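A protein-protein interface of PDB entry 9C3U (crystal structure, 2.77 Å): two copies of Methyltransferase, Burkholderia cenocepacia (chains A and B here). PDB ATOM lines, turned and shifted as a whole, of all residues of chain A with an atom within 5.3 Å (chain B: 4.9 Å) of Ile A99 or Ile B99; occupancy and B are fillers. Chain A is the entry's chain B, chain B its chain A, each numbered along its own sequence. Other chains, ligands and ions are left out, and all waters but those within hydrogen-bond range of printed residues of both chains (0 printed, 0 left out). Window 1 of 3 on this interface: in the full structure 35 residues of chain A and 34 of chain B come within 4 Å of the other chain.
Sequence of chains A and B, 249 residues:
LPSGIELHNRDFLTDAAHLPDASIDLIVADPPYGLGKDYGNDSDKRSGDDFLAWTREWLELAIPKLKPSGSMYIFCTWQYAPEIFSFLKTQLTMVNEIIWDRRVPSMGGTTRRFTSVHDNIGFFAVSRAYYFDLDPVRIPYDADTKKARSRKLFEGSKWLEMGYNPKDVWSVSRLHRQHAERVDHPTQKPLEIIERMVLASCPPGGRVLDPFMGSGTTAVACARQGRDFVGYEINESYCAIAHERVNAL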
ATOM      1  N   GLU A  97     -12.565 -17.794  -3.735  1.00  0.00           N
ATOM      2  CA  GLU A  97     -11.309 -17.443  -4.390  1.00  0.00           C
ATOM      3  C   GLU A  97     -10.255 -18.413  -3.871  1.00  0.00           C
ATOM      4  O   GLU A  97      -9.687 -18.210  -2.793  1.00  0.00           O
ATOM      5  CB  GLU A  97     -10.925 -15.995  -4.122  1.00  0.00           C
ATOM      6  CG  GLU A  97     -10.030 -15.395  -5.192  1.00  0.00           C
ATOM      7  CD  GLU A  97      -8.638 -15.089  -4.686  1.00  0.00           C
ATOM      8  OE1 GLU A  97      -8.498 -14.820  -3.477  1.00  0.00           O
ATOM      9  OE2 GLU A  97      -7.686 -15.119  -5.494  1.00  0.00           O
ATOM     10  N   ILE A  98      -9.970 -19.435  -4.671  1.00  0.00           N
ATOM     11  CA  ILE A  98      -9.005 -20.485  -4.248  1.00  0.00           C
ATOM     12  C   ILE A  98      -7.599 -20.074  -4.697  1.00  0.00           C
ATOM     13  O   ILE A  98      -7.439 -19.674  -5.856  1.00  0.00           O
ATOM     14  CB  ILE A  98      -9.427 -21.864  -4.785  1.00  0.00           C
ATOM     15  CG1 ILE A  98     -10.648 -22.396  -4.051  1.00  0.00           C
ATOM     16  CG2 ILE A  98      -8.264 -22.850  -4.728  1.00  0.00           C
ATOM     17  CD1 ILE A  98     -11.918 -22.369  -4.878  1.00  0.00           C
ATOM     18  N   ILE A  99      -6.645 -20.140  -3.778  1.00  0.00           N
ATOM     19  CA  ILE A  99      -5.236 -19.800  -4.111  1.00  0.00           C
ATOM     20  C   ILE A  99      -4.463 -21.112  -4.273  1.00  0.00           C
ATOM     21  O   ILE A  99      -4.434 -21.897  -3.319  1.00  0.00           O
ATOM     22  CB  ILE A  99      -4.639 -18.873  -3.039  1.00  0.00           C
ATOM     23  CG1 ILE A  99      -5.098 -17.451  -3.256  1.00  0.00           C
ATOM     24  CG2 ILE A  99      -3.115 -18.965  -3.013  1.00  0.00           C
ATOM     25  CD1 ILE A  99      -4.732 -16.907  -4.621  1.00  0.00           C
ATOM     26  N   TRP A 100      -3.908 -21.343  -5.461  1.00  0.00           N
ATOM     27  CA  TRP A 100      -3.077 -22.551  -5.652  1.00  0.00           C
ATOM     28  C   TRP A 100      -1.637 -22.256  -5.271  1.00  0.00           C
ATOM     29  O   TRP A 100      -0.917 -21.633  -6.059  1.00  0.00           O
ATOM     30  CB  TRP A 100      -3.156 -23.101  -7.080  1.00  0.00           C
ATOM     31  CG  TRP A 100      -2.192 -24.231  -7.328  1.00  0.00           C
ATOM     32  CD1 TRP A 100      -1.799 -25.188  -6.441  1.00  0.00           C
ATOM     33  CD2 TRP A 100      -1.481 -24.506  -8.552  1.00  0.00           C
ATOM     34  NE1 TRP A 100      -0.896 -26.034  -7.021  1.00  0.00           N
ATOM     35  CE2 TRP A 100      -0.683 -25.645  -8.315  1.00  0.00           C
ATOM     36  CE3 TRP A 100      -1.444 -23.910  -9.815  1.00  0.00           C
ATOM     37  CZ2 TRP A 100       0.141 -26.190  -9.293  1.00  0.00           C
ATOM     38  CZ3 TRP A 100      -0.631 -24.454 -10.782  1.00  0.00           C
ATOM     39  CH2 TRP A 100       0.150 -25.576 -10.523  1.00  0.00           C
ATOM     40  N   ASP A 101      -1.243 -22.698  -4.086  1.00  0.00           N
ATOM     41  CA  ASP A 101       0.151 -22.583  -3.673  1.00  0.00           C
ATOM     42  C   ASP A 101       0.935 -23.653  -4.419  1.00  0.00           C
ATOM     43  O   ASP A 101       0.920 -24.828  -4.044  1.00  0.00           O
ATOM     44  CB  ASP A 101       0.266 -22.752  -2.162  1.00  0.00           C
ATOM     45  CG  ASP A 101       1.672 -22.506  -1.632  1.00  0.00           C
ATOM     46  OD1 ASP A 101       2.661 -22.908  -2.281  1.00  0.00           O
ATOM     47  OD2 ASP A 101       1.785 -21.916  -0.539  1.00  0.00           O
ATOM     48  N   HIS A 118       1.956 -18.580  -6.423  1.00  0.00           N
ATOM     49  CA  HIS A 118       0.488 -18.673  -6.252  1.00  0.00           C
ATOM     50  C   HIS A 118      -0.218 -18.453  -7.580  1.00  0.00           C
ATOM     51  O   HIS A 118       0.207 -17.596  -8.370  1.00  0.00           O
ATOM     52  CB  HIS A 118      -0.020 -17.708  -5.171  1.00  0.00           C
ATOM     53  CG  HIS A 118      -0.510 -16.383  -5.635  1.00  0.00           C
ATOM     54  ND1 HIS A 118       0.267 -15.250  -5.577  1.00  0.00           N
ATOM     55  CD2 HIS A 118      -1.687 -15.998  -6.131  1.00  0.00           C
ATOM     56  CE1 HIS A 118      -0.423 -14.225  -6.048  1.00  0.00           C
ATOM     57  NE2 HIS A 118      -1.614 -14.657  -6.389  1.00  0.00           N
ATOM     58  N   ASP A 119      -1.256 -19.243  -7.823  1.00  0.00           N
ATOM     59  CA  ASP A 119      -2.098 -18.988  -9.017  1.00  0.00           C
ATOM     60  C   ASP A 119      -3.513 -18.772  -8.490  1.00  0.00           C
ATOM     61  O   ASP A 119      -3.886 -19.448  -7.524  1.00  0.00           O
ATOM     62  CB  ASP A 119      -1.990 -20.111 -10.031  1.00  0.00           C
ATOM     63  CG  ASP A 119      -0.781 -20.094 -10.950  1.00  0.00           C
ATOM     64  OD1 ASP A 119      -0.009 -19.124 -10.889  1.00  0.00           O
ATOM     65  OD2 ASP A 119      -0.629 -21.055 -11.725  1.00  0.00           O
ATOM     66  N   ASN A 120      -4.267 -17.858  -9.082  1.00  0.00           N
ATOM     67  CA  ASN A 120      -5.592 -17.530  -8.577  1.00  0.00           C
ATOM     68  C   ASN A 120      -6.639 -18.361  -9.304  1.00  0.00           C
ATOM     69  O   ASN A 120      -6.535 -18.588 -10.511  1.00  0.00           O
ATOM     70  CB  ASN A 120      -5.888 -16.039  -8.747  1.00  0.00           C
ATOM     71  CG  ASN A 120      -4.928 -15.163  -7.966  1.00  0.00           C
ATOM     72  OD1 ASN A 120      -3.751 -15.048  -8.313  1.00  0.00           O
ATOM     73  ND2 ASN A 120      -5.425 -14.541  -6.902  1.00  0.00           N
ATOM     74  N   ILE A 121      -7.644 -18.825  -8.564  1.00  0.00           N
ATOM     75  CA  ILE A 121      -8.744 -19.592  -9.128  1.00  0.00           C
ATOM     76  C   ILE A 121     -10.039 -18.960  -8.649  1.00  0.00           C
ATOM     77  O   ILE A 121     -10.276 -18.861  -7.440  1.00  0.00           O
ATOM     78  CB  ILE A 121      -8.687 -21.076  -8.729  1.00  0.00           C
ATOM     79  CG1 ILE A 121      -7.361 -21.703  -9.162  1.00  0.00           C
ATOM     80  CG2 ILE A 121      -9.853 -21.831  -9.345  1.00  0.00           C
ATOM     81  CD1 ILE A 121      -7.079 -23.037  -8.507  1.00  0.00           C
ATOM     82  N   ASP A 168      -9.688 -22.557   1.101  1.00  0.00           N
ATOM     83  CA  ASP A 168      -9.503 -21.846  -0.154  1.00  0.00           C
ATOM     84  C   ASP A 168      -8.033 -21.642  -0.503  1.00  0.00           C
ATOM     85  O   ASP A 168      -7.714 -20.777  -1.327  1.00  0.00           O
ATOM     86  CB  ASP A 168     -10.230 -20.498  -0.114  1.00  0.00           C
ATOM     87  CG  ASP A 168      -9.967 -19.728   1.164  1.00  0.00           C
ATOM     88  OD1 ASP A 168      -9.331 -20.287   2.081  1.00  0.00           O
ATOM     89  OD2 ASP A 168     -10.375 -18.548   1.238  1.00  0.00           O
ATOM     90  N   VAL A 169      -7.132 -22.402   0.116  1.00  0.00           N
ATOM     91  CA  VAL A 169      -5.712 -22.396  -0.221  1.00  0.00           C
ATOM     92  C   VAL A 169      -5.251 -23.841  -0.323  1.00  0.00           C
ATOM     93  O   VAL A 169      -5.348 -24.597   0.652  1.00  0.00           O
ATOM     94  CB  VAL A 169      -4.863 -21.630   0.807  1.00  0.00           C
ATOM     95  CG1 VAL A 169      -3.418 -21.555   0.342  1.00  0.00           C
ATOM     96  CG2 VAL A 169      -5.408 -20.240   0.995  1.00  0.00           C
ATOM     97  N   TRP A 170      -4.753 -24.223  -1.495  1.00  0.00           N
ATOM     98  CA  TRP A 170      -4.360 -25.596  -1.788  1.00  0.00           C
ATOM     99  C   TRP A 170      -2.855 -25.619  -2.013  1.00  0.00           C
ATOM    100  O   TRP A 170      -2.372 -25.138  -3.044  1.00  0.00           O
ATOM    101  CB  TRP A 170      -5.112 -26.126  -3.009  1.00  0.00           C
ATOM    102  CG  TRP A 170      -6.607 -26.069  -2.863  1.00  0.00           C
ATOM    103  CD1 TRP A 170      -7.312 -25.804  -1.723  1.00  0.00           C
ATOM    104  CD2 TRP A 170      -7.579 -26.268  -3.895  1.00  0.00           C
ATOM    105  NE1 TRP A 170      -8.660 -25.831  -1.981  1.00  0.00           N
ATOM    106  CE2 TRP A 170      -8.851 -26.116  -3.307  1.00  0.00           C
ATOM    107  CE3 TRP A 170      -7.499 -26.565  -5.259  1.00  0.00           C
ATOM    108  CZ2 TRP A 170     -10.031 -26.246  -4.035  1.00  0.00           C
ATOM    109  CZ3 TRP A 170      -8.671 -26.695  -5.980  1.00  0.00           C
ATOM    110  CH2 TRP A 170      -9.921 -26.536  -5.366  1.00  0.00           C
ATOM    111  N   GLU B  97       0.738  -9.335  -5.506  1.00  0.00           N
ATOM    112  CA  GLU B  97      -0.408  -9.760  -4.710  1.00  0.00           C
ATOM    113  C   GLU B  97       0.108 -10.792  -3.719  1.00  0.00           C
ATOM    114  O   GLU B  97       0.560 -11.871  -4.115  1.00  0.00           O
ATOM    115  CB  GLU B  97      -1.529 -10.332  -5.579  1.00  0.00           C
ATOM    116  CG  GLU B  97      -2.387 -11.366  -4.861  1.00  0.00           C
ATOM    117  CD  GLU B  97      -3.842 -11.321  -5.277  1.00  0.00           C
ATOM    118  OE1 GLU B  97      -4.712 -11.338  -4.381  1.00  0.00           O
ATOM    119  OE2 GLU B  97      -4.115 -11.272  -6.495  1.00  0.00           O
ATOM    120  N   ILE B  98       0.064 -10.441  -2.437  1.00  0.00           N
ATOM    121  CA  ILE B  98       0.603 -11.341  -1.380  1.00  0.00           C
ATOM    122  C   ILE B  98      -0.568 -12.021  -0.662  1.00  0.00           C
ATOM    123  O   ILE B  98      -1.558 -11.334  -0.367  1.00  0.00           O
ATOM    124  CB  ILE B  98       1.509 -10.562  -0.409  1.00  0.00           C
ATOM    125  CG1 ILE B  98       2.881 -10.294  -1.015  1.00  0.00           C
ATOM    126  CG2 ILE B  98       1.616 -11.273   0.939  1.00  0.00           C
ATOM    127  CD1 ILE B  98       3.181  -8.823  -1.231  1.00  0.00           C
ATOM    128  N   ILE B  99      -0.458 -13.331  -0.433  1.00  0.00           N
ATOM    129  CA  ILE B  99      -1.555 -14.095   0.229  1.00  0.00           C
ATOM    130  C   ILE B  99      -1.125 -14.451   1.652  1.00  0.00           C
ATOM    131  O   ILE B  99      -0.139 -15.180   1.813  1.00  0.00           O
ATOM    132  CB  ILE B  99      -1.968 -15.339  -0.572  1.00  0.00           C
ATOM    133  CG1 ILE B  99      -2.849 -14.945  -1.736  1.00  0.00           C
ATOM    134  CG2 ILE B  99      -2.651 -16.375   0.318  1.00  0.00           C
ATOM    135  CD1 ILE B  99      -2.089 -14.391  -2.923  1.00  0.00           C
ATOM    136  N   TRP B 100      -1.831 -13.899   2.635  1.00  0.00           N
ATOM    137  CA  TRP B 100      -1.544 -14.304   4.022  1.00  0.00           C
ATOM    138  C   TRP B 100      -2.293 -15.583   4.283  1.00  0.00           C
ATOM    139  O   TRP B 100      -3.504 -15.533   4.494  1.00  0.00           O
ATOM    140  CB  TRP B 100      -1.934 -13.237   5.048  1.00  0.00           C
ATOM    141  CG  TRP B 100      -1.764 -13.707   6.466  1.00  0.00           C
ATOM    142  CD1 TRP B 100      -0.850 -14.600   6.940  1.00  0.00           C
ATOM    143  CD2 TRP B 100      -2.555 -13.306   7.601  1.00  0.00           C
ATOM    144  NE1 TRP B 100      -1.018 -14.785   8.283  1.00  0.00           N
ATOM    145  CE2 TRP B 100      -2.053 -14.004   8.717  1.00  0.00           C
ATOM    146  CE3 TRP B 100      -3.628 -12.428   7.777  1.00  0.00           C
ATOM    147  CZ2 TRP B 100      -2.592 -13.851   9.988  1.00  0.00           C
ATOM    148  CZ3 TRP B 100      -4.154 -12.274   9.037  1.00  0.00           C
ATOM    149  CH2 TRP B 100      -3.647 -12.979  10.123  1.00  0.00           C
ATOM    150  N   ASP B 101      -1.601 -16.694   4.178  1.00  0.00           N
ATOM    151  CA  ASP B 101      -2.177 -17.978   4.567  1.00  0.00           C
ATOM    152  C   ASP B 101      -2.165 -18.018   6.086  1.00  0.00           C
ATOM    153  O   ASP B 101      -1.135 -18.287   6.709  1.00  0.00           O
ATOM    154  CB  ASP B 101      -1.394 -19.143   3.972  1.00  0.00           C
ATOM    155  CG  ASP B 101      -1.866 -20.498   4.491  1.00  0.00           C
ATOM    156  OD1 ASP B 101      -2.987 -20.586   5.040  1.00  0.00           O
ATOM    157  OD2 ASP B 101      -1.105 -21.479   4.357  1.00  0.00           O
ATOM    158  N   HIS B 118      -7.269 -17.527   3.895  1.00  0.00           N
ATOM    159  CA  HIS B 118      -6.314 -16.493   3.421  1.00  0.00           C
ATOM    160  C   HIS B 118      -6.847 -15.068   3.266  1.00  0.00           C
ATOM    161  O   HIS B 118      -8.034 -14.880   2.957  1.00  0.00           O
ATOM    162  CB  HIS B 118      -5.759 -16.935   2.066  1.00  0.00           C
ATOM    163  CG  HIS B 118      -6.584 -16.590   0.880  1.00  0.00           C
ATOM    164  ND1 HIS B 118      -6.221 -15.588   0.012  1.00  0.00           N
ATOM    165  CD2 HIS B 118      -7.716 -17.101   0.404  1.00  0.00           C
ATOM    166  CE1 HIS B 118      -7.124 -15.498  -0.946  1.00  0.00           C
ATOM    167  NE2 HIS B 118      -8.041 -16.409  -0.728  1.00  0.00           N
ATOM    168  N   ASP B 119      -5.975 -14.082   3.497  1.00  0.00           N
ATOM    169  CA  ASP B 119      -6.284 -12.679   3.257  1.00  0.00           C
ATOM    170  C   ASP B 119      -5.480 -12.167   2.069  1.00  0.00           C
ATOM    171  O   ASP B 119      -4.333 -12.576   1.853  1.00  0.00           O
ATOM    172  CB  ASP B 119      -6.000 -11.816   4.492  1.00  0.00           C
ATOM    173  CG  ASP B 119      -6.962 -12.091   5.631  1.00  0.00           C
ATOM    174  OD1 ASP B 119      -7.697 -13.099   5.560  1.00  0.00           O
ATOM    175  OD2 ASP B 119      -6.995 -11.287   6.588  1.00  0.00           O
ATOM    176  N   ASP B 168       5.075 -14.671  -2.720  1.00  0.00           N
ATOM    177  CA  ASP B 168       3.850 -13.907  -2.547  1.00  0.00           C
ATOM    178  C   ASP B 168       2.758 -14.679  -1.809  1.00  0.00           C
ATOM    179  O   ASP B 168       1.594 -14.265  -1.845  1.00  0.00           O
ATOM    180  CB  ASP B 168       3.340 -13.411  -3.901  1.00  0.00           C
ATOM    181  CG  ASP B 168       3.271 -14.508  -4.937  1.00  0.00           C
ATOM    182  OD1 ASP B 168       3.575 -15.670  -4.601  1.00  0.00           O
ATOM    183  OD2 ASP B 168       2.914 -14.207  -6.096  1.00  0.00           O
ATOM    184  N   VAL B 169       3.095 -15.780  -1.136  1.00  0.00           N
ATOM    185  CA  VAL B 169       2.209 -16.353  -0.128  1.00  0.00           C
ATOM    186  C   VAL B 169       3.024 -16.484   1.148  1.00  0.00           C
ATOM    187  O   VAL B 169       4.068 -17.147   1.160  1.00  0.00           O
ATOM    188  CB  VAL B 169       1.621 -17.722  -0.523  1.00  0.00           C
ATOM    189  CG1 VAL B 169       0.605 -17.584  -1.649  1.00  0.00           C
ATOM    190  CG2 VAL B 169       2.686 -18.747  -0.812  1.00  0.00           C
ATOM    191  N   TRP B 170       2.561 -15.844   2.208  1.00  0.00           N
ATOM    192  CA  TRP B 170       3.218 -15.879   3.505  1.00  0.00           C
ATOM    193  C   TRP B 170       2.387 -16.787   4.404  1.00  0.00           C
ATOM    194  O   TRP B 170       1.242 -16.461   4.733  1.00  0.00           O
ATOM    195  CB  TRP B 170       3.347 -14.468   4.078  1.00  0.00           C
ATOM    196  CG  TRP B 170       4.047 -13.496   3.151  1.00  0.00           C
ATOM    197  CD1 TRP B 170       4.636 -13.779   1.949  1.00  0.00           C
ATOM    198  CD2 TRP B 170       4.208 -12.085   3.348  1.00  0.00           C
ATOM    199  NE1 TRP B 170       5.160 -12.638   1.395  1.00  0.00           N
ATOM    200  CE2 TRP B 170       4.914 -11.584   2.234  1.00  0.00           C
ATOM    201  CE3 TRP B 170       3.832 -11.199   4.360  1.00  0.00           C
ATOM    202  CZ2 TRP B 170       5.244 -10.236   2.103  1.00  0.00           C
ATOM    203  CZ3 TRP B 170       4.163  -9.859   4.228  1.00  0.00           C
ATOM    204  CH2 TRP B 170       4.862  -9.393   3.109  1.00  0.00           C
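ND1 of His A118 sits at hydrogen-bond distance from OD2 of Asp B168, at 2.9 Å. The backbone carbonyl oxygen (O) of Glu A97 is in hydrogen-bond range of a ring nitrogen (NE2) of His B118, at 3.2 Å.
The backbone NH (N) of Asp A101 is in hydrogen-bond range of the backbone carbonyl oxygen (O) of Trp A170 (2.9 Å). O of Asp A168 is in hydrogen-bond range of N of Ile A99, 2.7 Å away. The backbone NH (N) of Ile B99 is in hydrogen-bond range of the backbone carbonyl oxygen (O) of Asp B168, at 2.7 Å. The backbone carbonyl oxygen (O) of Ile B99 is in hydrogen-bond range of the backbone NH (N) of Trp B170 (2.8 Å). O of Ile A99 lies within hydrogen-bond range of N of Trp A170 (3.0 Å). OE2 of Glu A97 is in hydrogen-bond range of ND2 of Asn A120, 2.7 Å away.
Ile A99 touches Ile B99 (CG1 to CG1, 3.7 Å). CG1 of Ile A99 touches CE1 of His B118, at 3.6 Å. Asp A101 touches Val B169. His A118 touches Glu B97 (CE1 to O, 3.2 Å). CD1 of Ile B99 touches NE2 of His A118, 3.5 Å away. His A118 touches Val B169. Glu B97 touches Asn A120 (OE2 to ND2, 3.5 Å). Asp A168 touches His B118. Val A169 touches His B118 (CG2 to CB, 3.5 Å).
Printed residues of chain B within 4 Å of Ile A99: Ile B99 (3.7 Å) and His B118 (3.6 Å). Ile B99 touches just these residues of chain A: Ile A99 (3.7 Å) and His A118 (3.5 Å). Printed residues of chain A within 4 Å of Val B169: Asp A101 and His A118. Printed residues of chain B within 4 Å of Val A169: His B118 (3.5 Å). Asp B101 touches none of the printed residues of chain A. The nearest residue of chain B that does not touch Ile A99 is Val B169 (4.2 Å). The nearest residue of chain A that does not touch Ile B99 is Val A169 (4.8 Å).
Hydrophobic or aromatic side chains of chain B within 4 Å of the printed part of chain A: Ile B99, His B118 and Val B169. Hydrophobic or aromatic side chains of chain A that line the printed part of chain B: Ile A99, His A118 and Val A169. Among the printed residues, 11 pairs touch across the chains. Among the printed residues, no Asp or Glu carboxylate lies within 4 Å of a Lys or Arg side-chain nitrogen of the other chain.
Glu A97 touches His B118, and with the chains exchanged His A118 touches Glu B97. Ile B99 touches its own counterpart, Ile A99. Ile A99 touches His B118, and with the chains exchanged His A118 touches Ile B99. His A118 touches Val B169, and with the chains exchanged Val A169 touches His B118. 10 positions are printed for both chains. Of the 11 pairs that touch across the chains among the printed residues, 9 have their exchanged pair printed and touching as well.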
